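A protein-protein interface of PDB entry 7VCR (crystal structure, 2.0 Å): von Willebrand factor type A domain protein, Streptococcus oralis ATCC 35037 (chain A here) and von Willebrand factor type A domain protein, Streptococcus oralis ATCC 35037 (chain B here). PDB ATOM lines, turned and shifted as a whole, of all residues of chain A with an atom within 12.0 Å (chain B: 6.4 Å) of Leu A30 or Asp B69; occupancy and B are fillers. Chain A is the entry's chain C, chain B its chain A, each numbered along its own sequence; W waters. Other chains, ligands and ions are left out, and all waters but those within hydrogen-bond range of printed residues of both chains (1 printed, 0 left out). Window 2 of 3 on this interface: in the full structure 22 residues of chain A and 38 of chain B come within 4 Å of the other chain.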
ATOM      1  N   GLU A   1      12.464  14.477  27.029  1.00  0.00           N
ATOM      2  CA  GLU A   1      12.639  14.369  25.538  1.00  0.00           C
ATOM      3  C   GLU A   1      12.571  12.913  25.063  1.00  0.00           C
ATOM      4  O   GLU A   1      13.076  12.005  25.724  1.00  0.00           O
ATOM      5  CB  GLU A   1      13.986  14.950  25.106  1.00  0.00           C
ATOM      6  CG  GLU A   1      15.201  14.152  25.528  1.00  0.00           C
ATOM      7  CD  GLU A   1      16.472  14.518  24.772  1.00  0.00           C
ATOM      8  OE1 GLU A   1      16.431  14.692  23.532  1.00  0.00           O
ATOM      9  OE2 GLU A   1      17.513  14.627  25.423  1.00  0.00           O
ATOM     10  N   PRO A   2      11.904  12.619  23.926  1.00  0.00           N
ATOM     11  CA  PRO A   2      11.923  11.253  23.366  1.00  0.00           C
ATOM     12  C   PRO A   2      13.325  10.697  23.095  1.00  0.00           C
ATOM     13  O   PRO A   2      14.271  11.438  22.861  1.00  0.00           O
ATOM     14  CB  PRO A   2      10.956  11.312  22.178  1.00  0.00           C
ATOM     15  CG  PRO A   2      10.055  12.510  22.489  1.00  0.00           C
ATOM     16  CD  PRO A   2      10.970  13.510  23.212  1.00  0.00           C
ATOM     17  N   GLN A   3      13.482   9.389  23.282  1.00  0.00           N
ATOM     18  CA  GLN A   3      14.716   8.696  22.980  1.00  0.00           C
ATOM     19  C   GLN A   3      14.614   8.242  21.511  1.00  0.00           C
ATOM     20  O   GLN A   3      13.567   7.721  21.074  1.00  0.00           O
ATOM     21  CB  GLN A   3      14.834   7.432  23.849  1.00  0.00           C
ATOM     22  CG  GLN A   3      14.766   7.669  25.362  1.00  0.00           C
ATOM     23  CD  GLN A   3      15.936   8.469  25.890  1.00  0.00           C
ATOM     24  OE1 GLN A   3      17.095   8.169  25.616  1.00  0.00           O
ATOM     25  NE2 GLN A   3      15.648   9.527  26.629  1.00  0.00           N
ATOM     26  N   THR A   4      15.719   8.394  20.781  1.00  0.00           N
ATOM     27  CA  THR A   4      15.741   7.991  19.377  1.00  0.00           C
ATOM     28  C   THR A   4      16.950   7.119  19.140  1.00  0.00           C
ATOM     29  O   THR A   4      17.991   7.374  19.709  1.00  0.00           O
ATOM     30  CB  THR A   4      15.800   9.200  18.426  1.00  0.00           C
ATOM     31  OG1 THR A   4      16.971   9.966  18.710  1.00  0.00           O
ATOM     32  CG2 THR A   4      14.612  10.128  18.596  1.00  0.00           C
ATOM     33  N   THR A   5      16.802   6.101  18.281  1.00  0.00           N
ATOM     34  CA  THR A   5      17.961   5.336  17.902  1.00  0.00           C
ATOM     35  C   THR A   5      18.055   5.360  16.359  1.00  0.00           C
ATOM     36  O   THR A   5      17.038   5.426  15.683  1.00  0.00           O
ATOM     37  CB  THR A   5      17.932   3.934  18.522  1.00  0.00           C
ATOM     38  OG1 THR A   5      16.824   3.294  17.907  1.00  0.00           O
ATOM     39  CG2 THR A   5      17.647   3.931  20.013  1.00  0.00           C
ATOM     40  N   ILE A  26      15.289   5.611  11.698  1.00  0.00           N
ATOM     41  CA  ILE A  26      15.123   6.271  12.975  1.00  0.00           C
ATOM     42  C   ILE A  26      13.934   5.584  13.672  1.00  0.00           C
ATOM     43  O   ILE A  26      12.912   5.356  13.029  1.00  0.00           O
ATOM     44  CB  ILE A  26      14.885   7.775  12.823  1.00  0.00           C
ATOM     45  CG1 ILE A  26      14.693   8.378  14.233  1.00  0.00           C
ATOM     46  CG2 ILE A  26      13.685   8.159  11.963  1.00  0.00           C
ATOM     47  CD1 ILE A  26      15.016   9.845  14.259  1.00  0.00           C
ATOM     48  N   THR A  27      14.083   5.290  14.961  1.00  0.00           N
ATOM     49  CA  THR A  27      12.974   4.835  15.808  1.00  0.00           C
ATOM     50  C   THR A  27      12.898   5.743  17.043  1.00  0.00           C
ATOM     51  O   THR A  27      13.939   6.060  17.630  1.00  0.00           O
ATOM     52  CB  THR A  27      13.261   3.426  16.383  1.00  0.00           C
ATOM     53  OG1 THR A  27      13.438   2.573  15.271  1.00  0.00           O
ATOM     54  CG2 THR A  27      12.118   2.794  17.155  1.00  0.00           C
ATOM     55  N   SER A  28      11.670   6.123  17.429  1.00  0.00           N
ATOM     56  CA  SER A  28      11.465   7.055  18.523  1.00  0.00           C
ATOM     57  C   SER A  28      10.621   6.400  19.624  1.00  0.00           C
ATOM     58  O   SER A  28       9.621   5.752  19.312  1.00  0.00           O
ATOM     59  CB  SER A  28      10.768   8.272  18.040  1.00  0.00           C
ATOM     60  OG  SER A  28      10.575   9.183  19.136  1.00  0.00           O
ATOM     61  N   LYS A  29      11.028   6.589  20.892  1.00  0.00           N
ATOM     62  CA  LYS A  29      10.274   6.142  22.071  1.00  0.00           C
ATOM     63  C   LYS A  29       9.915   7.350  22.945  1.00  0.00           C
ATOM     64  O   LYS A  29      10.770   8.202  23.141  1.00  0.00           O
ATOM     65  CB  LYS A  29      11.135   5.206  22.924  1.00  0.00           C
ATOM     66  CG  LYS A  29      10.496   3.879  23.330  1.00  0.00           C
ATOM     67  CD  LYS A  29      10.683   3.585  24.825  1.00  0.00           C
ATOM     68  CE  LYS A  29      12.139   3.534  25.255  1.00  0.00           C
ATOM     69  NZ  LYS A  29      12.570   2.145  25.552  1.00  0.00           N
ATOM     70  N   LEU A  30       8.676   7.427  23.473  1.00  0.00           N
ATOM     71  CA  LEU A  30       8.128   8.624  24.131  1.00  0.00           C
ATOM     72  C   LEU A  30       8.958   9.050  25.356  1.00  0.00           C
ATOM     73  O   LEU A  30       9.509   8.153  26.059  1.00  0.00           O
ATOM     74  CB  LEU A  30       6.649   8.420  24.478  1.00  0.00           C
ATOM     75  N   LYS B  31       6.069  -1.379  11.951  1.00  0.00           N
ATOM     76  CA  LYS B  31       5.512  -1.482  13.298  1.00  0.00           C
ATOM     77  C   LYS B  31       4.743  -2.787  13.399  1.00  0.00           C
ATOM     78  O   LYS B  31       3.932  -3.072  12.517  1.00  0.00           O
ATOM     79  CB  LYS B  31       4.576  -0.301  13.583  1.00  0.00           C
ATOM     80  CG  LYS B  31       4.087  -0.174  15.026  1.00  0.00           C
ATOM     81  CD  LYS B  31       5.204   0.035  16.032  1.00  0.00           C
ATOM     82  CE  LYS B  31       4.807  -0.181  17.496  1.00  0.00           C
ATOM     83  NZ  LYS B  31       4.010   0.916  18.055  1.00  0.00           N
ATOM     84  N   SER B  66       4.095  13.382  12.872  1.00  0.00           N
ATOM     85  CA  SER B  66       4.747  12.931  14.107  1.00  0.00           C
ATOM     86  C   SER B  66       5.050  11.451  13.986  1.00  0.00           C
ATOM     87  O   SER B  66       4.136  10.711  13.635  1.00  0.00           O
ATOM     88  CB  SER B  66       3.805  13.061  15.366  1.00  0.00           C
ATOM     89  OG  SER B  66       3.690  14.414  15.716  1.00  0.00           O
ATOM     90  N   LEU B  67       6.237  11.034  14.433  1.00  0.00           N
ATOM     91  CA  LEU B  67       6.582   9.626  14.314  1.00  0.00           C
ATOM     92  C   LEU B  67       5.784   8.843  15.347  1.00  0.00           C
ATOM     93  O   LEU B  67       5.725   9.248  16.484  1.00  0.00           O
ATOM     94  CB  LEU B  67       8.073   9.427  14.586  1.00  0.00           C
ATOM     95  CG  LEU B  67       9.022  10.158  13.628  1.00  0.00           C
ATOM     96  CD1 LEU B  67      10.427   9.605  13.801  1.00  0.00           C
ATOM     97  CD2 LEU B  67       8.611  10.077  12.163  1.00  0.00           C
ATOM     98  N   GLU B  68       5.135   7.762  14.904  1.00  0.00           N
ATOM     99  CA  GLU B  68       4.417   6.868  15.791  1.00  0.00           C
ATOM    100  C   GLU B  68       5.400   6.249  16.763  1.00  0.00           C
ATOM    101  O   GLU B  68       6.494   5.813  16.388  1.00  0.00           O
ATOM    102  CB  GLU B  68       3.656   5.841  14.972  1.00  0.00           C
ATOM    103  CG  GLU B  68       2.928   4.854  15.842  1.00  0.00           C
ATOM    104  CD  GLU B  68       2.289   3.685  15.131  1.00  0.00           C
ATOM    105  OE1 GLU B  68       2.355   3.657  13.883  1.00  0.00           O
ATOM    106  OE2 GLU B  68       1.706   2.813  15.834  1.00  0.00           O
ATOM    107  N   ASP B  69       5.012   6.225  18.038  1.00  0.00           N
ATOM    108  CA  ASP B  69       5.784   5.610  19.121  1.00  0.00           C
ATOM    109  C   ASP B  69       6.223   4.181  18.820  1.00  0.00           C
ATOM    110  O   ASP B  69       5.415   3.351  18.472  1.00  0.00           O
ATOM    111  CB  ASP B  69       4.981   5.610  20.437  1.00  0.00           C
ATOM    112  CG  ASP B  69       5.919   5.546  21.627  1.00  0.00           C
ATOM    113  OD1 ASP B  69       6.635   6.542  21.863  1.00  0.00           O
ATOM    114  OD2 ASP B  69       5.988   4.475  22.262  1.00  0.00           O
ATOM    115  N   GLY B  70       7.534   3.927  18.935  1.00  0.00           N
ATOM    116  CA  GLY B  70       8.108   2.603  18.747  1.00  0.00           C
ATOM    117  C   GLY B  70       8.142   2.132  17.282  1.00  0.00           C
ATOM    118  O   GLY B  70       8.592   1.027  17.048  1.00  0.00           O
ATOM    119  N   ALA B  71       7.694   2.944  16.294  1.00  0.00           N
ATOM    120  CA  ALA B  71       7.724   2.474  14.909  1.00  0.00           C
ATOM    121  C   ALA B  71       9.102   2.763  14.340  1.00  0.00           C
ATOM    122  O   ALA B  71       9.665   3.821  14.614  1.00  0.00           O
ATOM    123  CB  ALA B  71       6.671   3.166  14.062  1.00  0.00           C
ATOM    124  N   TYR B  73      11.115   3.998  11.187  1.00  0.00           N
ATOM    125  CA  TYR B  73      10.998   4.679   9.873  1.00  0.00           C
ATOM    126  C   TYR B  73      12.347   4.579   9.173  1.00  0.00           C
ATOM    127  O   TYR B  73      13.353   4.804   9.822  1.00  0.00           O
ATOM    128  CB  TYR B  73      10.687   6.166  10.049  1.00  0.00           C
ATOM    129  CG  TYR B  73       9.290   6.387  10.577  1.00  0.00           C
ATOM    130  CD1 TYR B  73       9.007   6.270  11.947  1.00  0.00           C
ATOM    131  CD2 TYR B  73       8.235   6.599   9.718  1.00  0.00           C
ATOM    132  CE1 TYR B  73       7.733   6.494  12.416  1.00  0.00           C
ATOM    133  CE2 TYR B  73       6.947   6.864  10.190  1.00  0.00           C
ATOM    134  CZ  TYR B  73       6.697   6.762  11.552  1.00  0.00           C
ATOM    135  OH  TYR B  73       5.430   6.951  12.100  1.00  0.00           O
HETATM  136  O   HOH W   1       9.320   6.160  15.900  1.00  0.00           O
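Leu A30 touches one residue of chain B.
Printed residues of chain A within 4 Å of Asp B69: Ser A28 (3.8 Å), Lys A29 (3.5 Å) and Leu A30 (2.7 Å).
Of chain A, only Thr A27 (3.9 Å) and Ser A28 (2.8 Å) come within 4 Å of Gly B70.
Ala B71 touches just these residues of chain A: Ile A26 and Thr A27.
Of the printed residues of chain B, Thr A27 touches Gly B70 and Ala B71.
Printed residues of chain B within 4 Å of Ser A28: Asp B69 and Gly B70.
Printed residues of chain A within 4 Å of Tyr B73: Ile A26.
Ser B66 touches none of the printed residues of chain A.
Glu A1 touches none of the printed residues of chain B.
The nearest printed residue of chain B that does not touch Lys A29 is Gly B70 (4.7 Å).
Among the printed residues, merely in contact across the chains: Lys A29 with Asp B69, Thr A27 with Ala B71, Ser A28 with Asp B69, Ile A26 with Ala B71 and Thr A27 with Gly B70.
Hydrophobic or aromatic side chains of chain B within 4 Å of the printed part of chain A: Tyr B73.
Along chain B the printed residues that touch a printed residue of chain A span positions 69 to 73.
Of the 10 printed residues of chain A, 5 touch a printed residue of chain B.
Among the printed residues, 8 pairs touch across the chains.
Among the printed residues, no Asp or Glu carboxylate lies within 4 Å of a Lys or Arg side-chain nitrogen of the other chain.
The backbone carbonyl oxygen (O) of Thr A27 lies within hydrogen-bond range of the backbone NH (N) of Thr A5.
N of Glu B68 is in hydrogen-bond range of OH of Tyr B73 (2.9 Å).
The backbone carbonyl oxygen of Gln A3 sits at hydrogen-bond distance from the backbone NH of Lys A29.
The side-chain amino group (NZ) of Lys B31 lies within hydrogen-bond range of the backbone carbonyl oxygen (O) of Asp B69, at 2.8 Å.
Water W1 lies within hydrogen-bond range of O of Ala B71, N of Ser A28 and O of Glu B68.
The side-chain carboxylate (OD1) of Asp B69 lies within hydrogen-bond range of the backbone NH (N) of Leu A30.
N of Gly B70 sits at hydrogen-bond distance from O of Ser A28 (2.8 Å).
The backbone NH (N) of Ile A26 lies within hydrogen-bond range of the backbone carbonyl oxygen (O) of Tyr B73.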
